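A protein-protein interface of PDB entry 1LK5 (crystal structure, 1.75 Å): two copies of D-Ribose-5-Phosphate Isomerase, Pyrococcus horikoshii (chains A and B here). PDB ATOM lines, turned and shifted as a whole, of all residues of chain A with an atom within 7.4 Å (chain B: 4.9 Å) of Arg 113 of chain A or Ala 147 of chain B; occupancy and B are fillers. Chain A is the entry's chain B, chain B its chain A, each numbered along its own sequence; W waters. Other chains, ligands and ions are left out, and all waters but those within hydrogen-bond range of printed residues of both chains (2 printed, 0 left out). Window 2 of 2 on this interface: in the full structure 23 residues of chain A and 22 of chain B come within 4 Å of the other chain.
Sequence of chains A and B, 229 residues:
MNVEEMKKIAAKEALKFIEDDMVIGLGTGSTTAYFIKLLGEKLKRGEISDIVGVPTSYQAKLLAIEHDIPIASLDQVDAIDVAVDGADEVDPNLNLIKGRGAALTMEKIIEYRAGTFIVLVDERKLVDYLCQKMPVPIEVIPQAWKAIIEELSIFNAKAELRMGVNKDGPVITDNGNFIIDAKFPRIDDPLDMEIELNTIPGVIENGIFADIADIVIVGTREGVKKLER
Hydrophobic or aromatic side chains of chain A within 4 Å of the printed part of chain B: Ile 109 and Tyr 112. Hydrophobic or aromatic side chains of chain B within 4 Å of the printed part of chain A: Trp 145, Ala 147, Ile 148, Ile 200 and Pro 201.
NH1 of Arg 113 of chain A is in hydrogen-bond range of O of Ile 109 of chain A, 2.8 Å away.
No position is printed for both chains.
Val 82 of chain A touches none of the printed residues of chain B. Of the printed residues of chain B, Ile 109 of chain A touches Pro 201 (3.8 Å). Of the printed residues of chain B, Arg 113 of chain A touches Ala 147 (3.6 Å), Ile 148 (3.6 Å), Glu 151 (2.8 Å), Ile 200 (3.5 Å) and Pro 201 (3.0 Å). Gly 115 of chain A touches none of the printed residues of chain B. Of chain A, only Arg 113 comes within 4 Å of Ala 147 of chain B. Printed residues of chain A within 4 Å of Ile 200 of chain B: Arg 113.
Water W1 lies within hydrogen-bond range of the side-chain amino group of Lys 146 of chain B (2.7 Å), the backbone carbonyl oxygen of Asp 75 of chain A (2.9 Å) and the backbone carbonyl oxygen of Val 77 of chain A (3.4 Å). Water W2 bridges the side-chain hydroxyl (OH) of Tyr 112 of chain A (2.8 Å) and the side-chain carboxylate (OE2) of Glu 151 of chain B (2.8 Å).
The indole nitrogen (NE1) of Trp 145 of chain B sits at hydrogen-bond distance from the side-chain carboxylate (OD2) of Asp 75 of chain A (3.1 Å). The guanidinium group (NE) of Arg 113 of chain A lies within salt-bridge range of the side-chain carboxylate (OE1) of Glu 151 of chain B (2.8 Å). The backbone carbonyl oxygen (O) of Pro 201 of chain B is in hydrogen-bond range of the guanidinium group (NH1) of Arg 113 of chain A (3.0 Å).
Lys 146 of chain B touches Asp 75 of chain A (CD to O, 3.9 Å). Lys 108 of chain A touches Pro 201 of chain B. CG1 of Ile 109 of chain A touches C of Pro 201 of chain B, at 3.8 Å. Tyr 112 of chain A touches Glu 151 of chain B. CG of Pro 201 of chain B touches CG of Tyr 112 of chain A, at 3.6 Å. Arg 113 of chain A touches Ala 147 of chain B (NE to CB, 3.6 Å). Arg 113 of chain A touches Ile 148 of chain B. Arg 113 of chain A touches Ile 200 of chain B.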
ATOM      1  N   LEU A  74      -9.158 -21.714  -5.660  1.00  0.00           N
ATOM      2  CA  LEU A  74      -8.503 -22.993  -5.426  1.00  0.00           C
ATOM      3  C   LEU A  74      -6.980 -22.881  -5.374  1.00  0.00           C
ATOM      4  O   LEU A  74      -6.315 -23.551  -4.579  1.00  0.00           O
ATOM      5  CB  LEU A  74      -8.900 -23.996  -6.512  1.00  0.00           C
ATOM      6  CG  LEU A  74      -8.203 -25.348  -6.451  1.00  0.00           C
ATOM      7  CD1 LEU A  74      -8.506 -26.032  -5.142  1.00  0.00           C
ATOM      8  CD2 LEU A  74      -8.638 -26.222  -7.626  1.00  0.00           C
ATOM      9  N   ASP A  75      -6.424 -22.036  -6.235  1.00  0.00           N
ATOM     10  CA  ASP A  75      -4.990 -21.894  -6.328  1.00  0.00           C
ATOM     11  C   ASP A  75      -4.387 -21.074  -5.188  1.00  0.00           C
ATOM     12  O   ASP A  75      -3.171 -20.907  -5.115  1.00  0.00           O
ATOM     13  CB  ASP A  75      -4.593 -21.331  -7.693  1.00  0.00           C
ATOM     14  CG  ASP A  75      -5.191 -19.968  -7.972  1.00  0.00           C
ATOM     15  OD1 ASP A  75      -6.408 -19.737  -7.734  1.00  0.00           O
ATOM     16  OD2 ASP A  75      -4.493 -19.059  -8.463  1.00  0.00           O
ATOM     17  N   VAL A  77      -5.098 -21.966  -1.980  1.00  0.00           N
ATOM     18  CA  VAL A  77      -5.034 -22.892  -0.848  1.00  0.00           C
ATOM     19  C   VAL A  77      -4.220 -24.135  -1.150  1.00  0.00           C
ATOM     20  O   VAL A  77      -3.942 -24.445  -2.312  1.00  0.00           O
ATOM     21  CB  VAL A  77      -6.447 -23.307  -0.378  1.00  0.00           C
ATOM     22  CG1 VAL A  77      -7.296 -22.088  -0.120  1.00  0.00           C
ATOM     23  CG2 VAL A  77      -7.122 -24.221  -1.393  1.00  0.00           C
ATOM     24  N   ASP A  78      -3.836 -24.858  -0.104  1.00  0.00           N
ATOM     25  CA  ASP A  78      -2.982 -26.015  -0.272  1.00  0.00           C
ATOM     26  C   ASP A  78      -3.811 -27.293  -0.347  1.00  0.00           C
ATOM     27  O   ASP A  78      -3.332 -28.324  -0.838  1.00  0.00           O
ATOM     28  CB  ASP A  78      -1.965 -26.093   0.874  1.00  0.00           C
ATOM     29  CG  ASP A  78      -1.031 -24.882   0.917  1.00  0.00           C
ATOM     30  OD1 ASP A  78      -0.734 -24.300  -0.148  1.00  0.00           O
ATOM     31  OD2 ASP A  78      -0.546 -24.440   1.973  1.00  0.00           O
ATOM     32  N   ALA A  79      -5.058 -27.226   0.111  1.00  0.00           N
ATOM     33  CA  ALA A  79      -5.931 -28.394   0.078  1.00  0.00           C
ATOM     34  C   ALA A  79      -7.376 -28.020   0.325  1.00  0.00           C
ATOM     35  O   ALA A  79      -7.655 -27.002   0.937  1.00  0.00           O
ATOM     36  CB  ALA A  79      -5.487 -29.412   1.130  1.00  0.00           C
ATOM     37  N   ILE A  80      -8.289 -28.844  -0.180  1.00  0.00           N
ATOM     38  CA  ILE A  80      -9.702 -28.733   0.135  1.00  0.00           C
ATOM     39  C   ILE A  80      -9.990 -29.891   1.095  1.00  0.00           C
ATOM     40  O   ILE A  80      -9.886 -31.051   0.712  1.00  0.00           O
ATOM     41  CB  ILE A  80     -10.575 -28.896  -1.115  1.00  0.00           C
ATOM     42  CG1 ILE A  80     -10.248 -27.835  -2.178  1.00  0.00           C
ATOM     43  CG2 ILE A  80     -12.052 -28.856  -0.733  1.00  0.00           C
ATOM     44  CD1 ILE A  80     -10.677 -26.446  -1.823  1.00  0.00           C
ATOM     45  N   ASP A  81     -10.331 -29.591   2.341  1.00  0.00           N
ATOM     46  CA  ASP A  81     -10.591 -30.654   3.313  1.00  0.00           C
ATOM     47  C   ASP A  81     -11.942 -31.318   3.079  1.00  0.00           C
ATOM     48  O   ASP A  81     -12.055 -32.547   3.044  1.00  0.00           O
ATOM     49  CB  ASP A  81     -10.553 -30.094   4.736  1.00  0.00           C
ATOM     50  CG  ASP A  81      -9.204 -29.526   5.097  1.00  0.00           C
ATOM     51  OD1 ASP A  81      -8.203 -30.282   5.091  1.00  0.00           O
ATOM     52  OD2 ASP A  81      -9.032 -28.327   5.378  1.00  0.00           O
ATOM     53  N   VAL A  82     -12.974 -30.498   2.974  1.00  0.00           N
ATOM     54  CA  VAL A  82     -14.332 -30.970   2.769  1.00  0.00           C
ATOM     55  C   VAL A  82     -15.003 -30.061   1.731  1.00  0.00           C
ATOM     56  O   VAL A  82     -14.771 -28.856   1.724  1.00  0.00           O
ATOM     57  CB  VAL A  82     -15.147 -30.903   4.078  1.00  0.00           C
ATOM     58  CG1 VAL A  82     -16.587 -31.257   3.826  1.00  0.00           C
ATOM     59  CG2 VAL A  82     -14.538 -31.818   5.149  1.00  0.00           C
ATOM     60  N   ALA A  83     -15.763 -30.648   0.817  1.00  0.00           N
ATOM     61  CA  ALA A  83     -16.560 -29.874  -0.130  1.00  0.00           C
ATOM     62  C   ALA A  83     -18.014 -30.284   0.036  1.00  0.00           C
ATOM     63  O   ALA A  83     -18.333 -31.476   0.118  1.00  0.00           O
ATOM     64  CB  ALA A  83     -16.099 -30.084  -1.582  1.00  0.00           C
ATOM     65  N   THR A 105     -18.468 -26.690 -13.962  1.00  0.00           N
ATOM     66  CA  THR A 105     -17.033 -26.704 -14.143  1.00  0.00           C
ATOM     67  C   THR A 105     -16.272 -26.398 -12.853  1.00  0.00           C
ATOM     68  O   THR A 105     -15.408 -27.173 -12.441  1.00  0.00           O
ATOM     69  CB  THR A 105     -16.631 -25.736 -15.268  1.00  0.00           C
ATOM     70  OG1 THR A 105     -17.076 -26.283 -16.516  1.00  0.00           O
ATOM     71  CG2 THR A 105     -15.126 -25.663 -15.419  1.00  0.00           C
ATOM     72  N   MET A 106     -16.588 -25.278 -12.210  1.00  0.00           N
ATOM     73  CA  MET A 106     -15.877 -24.950 -10.981  1.00  0.00           C
ATOM     74  C   MET A 106     -16.230 -25.930  -9.856  1.00  0.00           C
ATOM     75  O   MET A 106     -15.393 -26.257  -9.015  1.00  0.00           O
ATOM     76  CB  MET A 106     -16.137 -23.529 -10.542  1.00  0.00           C
ATOM     77  CG  MET A 106     -15.112 -23.076  -9.532  1.00  0.00           C
ATOM     78  SD  MET A 106     -13.415 -23.015 -10.238  1.00  0.00           S
ATOM     79  CE  MET A 106     -12.584 -24.019  -9.062  1.00  0.00           C
ATOM     80  N   GLU A 107     -17.470 -26.398  -9.858  1.00  0.00           N
ATOM     81  CA  GLU A 107     -17.888 -27.416  -8.908  1.00  0.00           C
ATOM     82  C   GLU A 107     -16.991 -28.657  -9.006  1.00  0.00           C
ATOM     83  O   GLU A 107     -16.422 -29.126  -8.013  1.00  0.00           O
ATOM     84  CB  GLU A 107     -19.343 -27.784  -9.156  1.00  0.00           C
ATOM     85  CG  GLU A 107     -20.334 -26.735  -8.704  1.00  0.00           C
ATOM     86  CD  GLU A 107     -21.732 -26.917  -9.255  1.00  0.00           C
ATOM     87  OE1 GLU A 107     -22.009 -27.924  -9.959  1.00  0.00           O
ATOM     88  OE2 GLU A 107     -22.575 -26.039  -8.991  1.00  0.00           O
ATOM     89  N   LYS A 108     -16.833 -29.201 -10.204  1.00  0.00           N
ATOM     90  CA  LYS A 108     -16.010 -30.399 -10.317  1.00  0.00           C
ATOM     91  C   LYS A 108     -14.532 -30.107 -10.013  1.00  0.00           C
ATOM     92  O   LYS A 108     -13.835 -30.935  -9.417  1.00  0.00           O
ATOM     93  CB  LYS A 108     -16.210 -31.084 -11.676  1.00  0.00           C
ATOM     94  CG  LYS A 108     -15.879 -32.572 -11.605  1.00  0.00           C
ATOM     95  CD  LYS A 108     -16.146 -33.325 -12.890  1.00  0.00           C
ATOM     96  CE  LYS A 108     -17.606 -33.438 -13.225  1.00  0.00           C
ATOM     97  NZ  LYS A 108     -17.823 -34.173 -14.516  1.00  0.00           N
ATOM     98  N   ILE A 109     -14.042 -28.935 -10.416  1.00  0.00           N
ATOM     99  CA  ILE A 109     -12.672 -28.552 -10.134  1.00  0.00           C
ATOM    100  C   ILE A 109     -12.353 -28.618  -8.649  1.00  0.00           C
ATOM    101  O   ILE A 109     -11.334 -29.181  -8.262  1.00  0.00           O
ATOM    102  CB  ILE A 109     -12.361 -27.152 -10.675  1.00  0.00           C
ATOM    103  CG1 ILE A 109     -12.124 -27.209 -12.190  1.00  0.00           C
ATOM    104  CG2 ILE A 109     -11.126 -26.588 -10.019  1.00  0.00           C
ATOM    105  CD1 ILE A 109     -12.236 -25.837 -12.877  1.00  0.00           C
ATOM    106  N   ILE A 110     -13.253 -28.073  -7.839  1.00  0.00           N
ATOM    107  CA  ILE A 110     -13.060 -28.009  -6.404  1.00  0.00           C
ATOM    108  C   ILE A 110     -13.370 -29.350  -5.721  1.00  0.00           C
ATOM    109  O   ILE A 110     -12.608 -29.813  -4.896  1.00  0.00           O
ATOM    110  CB  ILE A 110     -13.936 -26.874  -5.843  1.00  0.00           C
ATOM    111  CG1 ILE A 110     -13.321 -25.526  -6.209  1.00  0.00           C
ATOM    112  CG2 ILE A 110     -14.053 -26.957  -4.339  1.00  0.00           C
ATOM    113  CD1 ILE A 110     -14.319 -24.404  -6.237  1.00  0.00           C
ATOM    114  N   GLU A 111     -14.456 -29.992  -6.124  1.00  0.00           N
ATOM    115  CA  GLU A 111     -14.922 -31.217  -5.461  1.00  0.00           C
ATOM    116  C   GLU A 111     -14.038 -32.415  -5.727  1.00  0.00           C
ATOM    117  O   GLU A 111     -13.909 -33.320  -4.891  1.00  0.00           O
ATOM    118  CB  GLU A 111     -16.376 -31.451  -5.851  1.00  0.00           C
ATOM    119  CG  GLU A 111     -17.263 -30.411  -5.175  1.00  0.00           C
ATOM    120  CD  GLU A 111     -18.507 -29.996  -5.929  1.00  0.00           C
ATOM    121  OE1 GLU A 111     -18.968 -30.712  -6.857  1.00  0.00           O
ATOM    122  OE2 GLU A 111     -19.051 -28.914  -5.558  1.00  0.00           O
ATOM    123  N   TYR A 112     -13.393 -32.406  -6.882  1.00  0.00           N
ATOM    124  CA  TYR A 112     -12.469 -33.460  -7.243  1.00  0.00           C
ATOM    125  C   TYR A 112     -11.284 -33.472  -6.290  1.00  0.00           C
ATOM    126  O   TYR A 112     -10.737 -34.523  -6.019  1.00  0.00           O
ATOM    127  CB  TYR A 112     -11.999 -33.245  -8.687  1.00  0.00           C
ATOM    128  CG  TYR A 112     -10.918 -34.160  -9.200  1.00  0.00           C
ATOM    129  CD1 TYR A 112     -11.206 -35.452  -9.608  1.00  0.00           C
ATOM    130  CD2 TYR A 112      -9.618 -33.701  -9.353  1.00  0.00           C
ATOM    131  CE1 TYR A 112     -10.210 -36.277 -10.113  1.00  0.00           C
ATOM    132  CE2 TYR A 112      -8.621 -34.513  -9.856  1.00  0.00           C
ATOM    133  CZ  TYR A 112      -8.929 -35.803 -10.239  1.00  0.00           C
ATOM    134  OH  TYR A 112      -7.934 -36.622 -10.744  1.00  0.00           O
ATOM    135  N   ARG A 113     -10.907 -32.307  -5.771  1.00  0.00           N
ATOM    136  CA  ARG A 113      -9.746 -32.214  -4.895  1.00  0.00           C
ATOM    137  C   ARG A 113     -10.084 -32.318  -3.406  1.00  0.00           C
ATOM    138  O   ARG A 113      -9.184 -32.245  -2.578  1.00  0.00           O
ATOM    139  CB  ARG A 113      -8.963 -30.920  -5.152  1.00  0.00           C
ATOM    140  CG  ARG A 113      -8.012 -30.992  -6.352  1.00  0.00           C
ATOM    141  CD  ARG A 113      -8.493 -30.267  -7.562  1.00  0.00           C
ATOM    142  NE  ARG A 113      -7.748 -30.621  -8.768  1.00  0.00           N
ATOM    143  CZ  ARG A 113      -8.161 -30.342  -9.999  1.00  0.00           C
ATOM    144  NH1 ARG A 113      -9.310 -29.703 -10.188  1.00  0.00           N
ATOM    145  NH2 ARG A 113      -7.436 -30.712 -11.048  1.00  0.00           N
ATOM    146  N   ALA A 114     -11.359 -32.509  -3.072  1.00  0.00           N
ATOM    147  CA  ALA A 114     -11.780 -32.570  -1.668  1.00  0.00           C
ATOM    148  C   ALA A 114     -11.455 -33.896  -0.979  1.00  0.00           C
ATOM    149  O   ALA A 114     -11.706 -34.965  -1.530  1.00  0.00           O
ATOM    150  CB  ALA A 114     -13.266 -32.326  -1.571  1.00  0.00           C
ATOM    151  N   GLY A 115     -10.946 -33.814   0.244  1.00  0.00           N
ATOM    152  CA  GLY A 115     -10.755 -34.994   1.077  1.00  0.00           C
ATOM    153  C   GLY A 115     -12.064 -35.745   1.248  1.00  0.00           C
ATOM    154  O   GLY A 115     -12.112 -36.969   1.134  1.00  0.00           O
ATOM    155  N   THR A 116     -13.132 -35.015   1.534  1.00  0.00           N
ATOM    156  CA  THR A 116     -14.472 -35.583   1.574  1.00  0.00           C
ATOM    157  C   THR A 116     -15.424 -34.678   0.798  1.00  0.00           C
ATOM    158  O   THR A 116     -15.494 -33.477   1.081  1.00  0.00           O
ATOM    159  CB  THR A 116     -14.976 -35.690   3.027  1.00  0.00           C
ATOM    160  OG1 THR A 116     -14.061 -36.470   3.803  1.00  0.00           O
ATOM    161  CG2 THR A 116     -16.296 -36.453   3.106  1.00  0.00           C
ATOM    162  N   ILE A 212     -17.362 -39.819  -7.351  1.00  0.00           N
ATOM    163  CA  ILE A 212     -16.749 -38.657  -6.700  1.00  0.00           C
ATOM    164  C   ILE A 212     -17.386 -38.321  -5.343  1.00  0.00           C
ATOM    165  O   ILE A 212     -16.685 -37.933  -4.420  1.00  0.00           O
ATOM    166  CB  ILE A 212     -16.771 -37.435  -7.657  1.00  0.00           C
ATOM    167  CG1 ILE A 212     -16.048 -36.240  -7.031  1.00  0.00           C
ATOM    168  CG2 ILE A 212     -18.179 -37.070  -8.059  1.00  0.00           C
ATOM    169  CD1 ILE A 212     -15.840 -35.112  -8.005  1.00  0.00           C
ATOM    170  N   ALA B 144      -7.468 -23.614 -11.525  1.00  0.00           N
ATOM    171  CA  ALA B 144      -7.030 -24.994 -11.413  1.00  0.00           C
ATOM    172  C   ALA B 144      -5.548 -25.173 -11.737  1.00  0.00           C
ATOM    173  O   ALA B 144      -5.023 -26.272 -11.619  1.00  0.00           O
ATOM    174  CB  ALA B 144      -7.865 -25.875 -12.338  1.00  0.00           C
ATOM    175  N   TRP B 145      -4.861 -24.100 -12.121  1.00  0.00           N
ATOM    176  CA  TRP B 145      -3.492 -24.229 -12.611  1.00  0.00           C
ATOM    177  C   TRP B 145      -2.512 -24.920 -11.655  1.00  0.00           C
ATOM    178  O   TRP B 145      -1.778 -25.822 -12.069  1.00  0.00           O
ATOM    179  CB  TRP B 145      -2.925 -22.874 -13.088  1.00  0.00           C
ATOM    180  CG  TRP B 145      -2.451 -22.003 -11.974  1.00  0.00           C
ATOM    181  CD1 TRP B 145      -3.187 -21.115 -11.272  1.00  0.00           C
ATOM    182  CD2 TRP B 145      -1.131 -21.954 -11.422  1.00  0.00           C
ATOM    183  NE1 TRP B 145      -2.414 -20.506 -10.312  1.00  0.00           N
ATOM    184  CE2 TRP B 145      -1.141 -21.000 -10.391  1.00  0.00           C
ATOM    185  CE3 TRP B 145       0.068 -22.606 -11.711  1.00  0.00           C
ATOM    186  CZ2 TRP B 145      -0.010 -20.697  -9.642  1.00  0.00           C
ATOM    187  CZ3 TRP B 145       1.185 -22.311 -10.961  1.00  0.00           C
ATOM    188  CH2 TRP B 145       1.140 -21.364  -9.945  1.00  0.00           C
ATOM    189  N   LYS B 146      -2.527 -24.534 -10.383  1.00  0.00           N
ATOM    190  CA  LYS B 146      -1.588 -25.076  -9.389  1.00  0.00           C
ATOM    191  C   LYS B 146      -1.847 -26.542  -9.045  1.00  0.00           C
ATOM    192  O   LYS B 146      -0.912 -27.325  -8.881  1.00  0.00           O
ATOM    193  CB  LYS B 146      -1.602 -24.197  -8.121  1.00  0.00           C
ATOM    194  CG  LYS B 146      -0.514 -24.540  -7.079  1.00  0.00           C
ATOM    195  CD  LYS B 146      -0.313 -23.398  -6.055  1.00  0.00           C
ATOM    196  CE  LYS B 146       0.851 -23.678  -5.114  1.00  0.00           C
ATOM    197  NZ  LYS B 146       1.054 -22.633  -4.036  1.00  0.00           N
ATOM    198  N   ALA B 147      -3.105 -26.931  -8.928  1.00  0.00           N
ATOM    199  CA  ALA B 147      -3.441 -28.308  -8.614  1.00  0.00           C
ATOM    200  C   ALA B 147      -3.085 -29.217  -9.779  1.00  0.00           C
ATOM    201  O   ALA B 147      -2.577 -30.330  -9.586  1.00  0.00           O
ATOM    202  CB  ALA B 147      -4.902 -28.432  -8.284  1.00  0.00           C
ATOM    203  N   ILE B 148      -3.330 -28.743 -10.992  1.00  0.00           N
ATOM    204  CA  ILE B 148      -3.059 -29.578 -12.150  1.00  0.00           C
ATOM    205  C   ILE B 148      -1.568 -29.840 -12.299  1.00  0.00           C
ATOM    206  O   ILE B 148      -1.164 -30.980 -12.572  1.00  0.00           O
ATOM    207  CB  ILE B 148      -3.678 -28.988 -13.420  1.00  0.00           C
ATOM    208  CG1 ILE B 148      -5.192 -29.156 -13.357  1.00  0.00           C
ATOM    209  CG2 ILE B 148      -3.108 -29.698 -14.640  1.00  0.00           C
ATOM    210  CD1 ILE B 148      -5.977 -28.359 -14.354  1.00  0.00           C
ATOM    211  N   ILE B 149      -0.753 -28.808 -12.118  1.00  0.00           N
ATOM    212  CA  ILE B 149       0.695 -28.979 -12.201  1.00  0.00           C
ATOM    213  C   ILE B 149       1.150 -30.034 -11.190  1.00  0.00           C
ATOM    214  O   ILE B 149       1.902 -30.952 -11.521  1.00  0.00           O
ATOM    215  CB  ILE B 149       1.424 -27.658 -11.933  1.00  0.00           C
ATOM    216  CG1 ILE B 149       1.313 -26.746 -13.160  1.00  0.00           C
ATOM    217  CG2 ILE B 149       2.888 -27.900 -11.609  1.00  0.00           C
ATOM    218  CD1 ILE B 149       2.048 -25.419 -13.031  1.00  0.00           C
ATOM    219  N   GLU B 150       0.690 -29.881  -9.953  1.00  0.00           N
ATOM    220  CA  GLU B 150       1.036 -30.835  -8.890  1.00  0.00           C
ATOM    221  C   GLU B 150       0.565 -32.245  -9.186  1.00  0.00           C
ATOM    222  O   GLU B 150       1.265 -33.225  -8.864  1.00  0.00           O
ATOM    223  CB  GLU B 150       0.452 -30.367  -7.558  1.00  0.00           C
ATOM    224  CG  GLU B 150       1.225 -29.202  -6.977  1.00  0.00           C
ATOM    225  CD  GLU B 150       0.536 -28.526  -5.808  1.00  0.00           C
ATOM    226  OE1 GLU B 150      -0.609 -28.911  -5.475  1.00  0.00           O
ATOM    227  OE2 GLU B 150       1.150 -27.601  -5.225  1.00  0.00           O
ATOM    228  N   GLU B 151      -0.619 -32.385  -9.767  1.00  0.00           N
ATOM    229  CA  GLU B 151      -1.146 -33.703 -10.042  1.00  0.00           C
ATOM    230  C   GLU B 151      -0.359 -34.415 -11.130  1.00  0.00           C
ATOM    231  O   GLU B 151      -0.226 -35.649 -11.106  1.00  0.00           O
ATOM    232  CB  GLU B 151      -2.627 -33.609 -10.383  1.00  0.00           C
ATOM    233  CG  GLU B 151      -3.441 -33.250  -9.148  1.00  0.00           C
ATOM    234  CD  GLU B 151      -4.783 -32.619  -9.442  1.00  0.00           C
ATOM    235  OE1 GLU B 151      -5.402 -32.116  -8.477  1.00  0.00           O
ATOM    236  OE2 GLU B 151      -5.227 -32.616 -10.609  1.00  0.00           O
ATOM    237  N   ILE B 200      -9.124 -34.715 -16.363  1.00  0.00           N
ATOM    238  CA  ILE B 200      -8.762 -33.953 -15.158  1.00  0.00           C
ATOM    239  C   ILE B 200      -9.630 -32.713 -15.082  1.00  0.00           C
ATOM    240  O   ILE B 200      -9.575 -31.900 -15.987  1.00  0.00           O
ATOM    241  CB  ILE B 200      -7.290 -33.516 -15.201  1.00  0.00           C
ATOM    242  CG1 ILE B 200      -6.355 -34.724 -15.157  1.00  0.00           C
ATOM    243  CG2 ILE B 200      -7.016 -32.523 -14.054  1.00  0.00           C
ATOM    244  CD1 ILE B 200      -4.916 -34.383 -15.440  1.00  0.00           C
ATOM    245  N   PRO B 201     -10.458 -32.564 -14.044  1.00  0.00           N
ATOM    246  CA  PRO B 201     -11.284 -31.363 -13.930  1.00  0.00           C
ATOM    247  C   PRO B 201     -10.434 -30.098 -13.953  1.00  0.00           C
ATOM    248  O   PRO B 201      -9.474 -29.953 -13.191  1.00  0.00           O
ATOM    249  CB  PRO B 201     -12.011 -31.559 -12.592  1.00  0.00           C
ATOM    250  CG  PRO B 201     -12.074 -33.041 -12.461  1.00  0.00           C
ATOM    251  CD  PRO B 201     -10.752 -33.528 -12.969  1.00  0.00           C
HETATM  252  O   HOH W   1      -1.478 -22.327  -3.183  1.00  0.00           O
HETATM  253  O   HOH W   2      -5.544 -35.338 -11.390  1.00  0.00           O
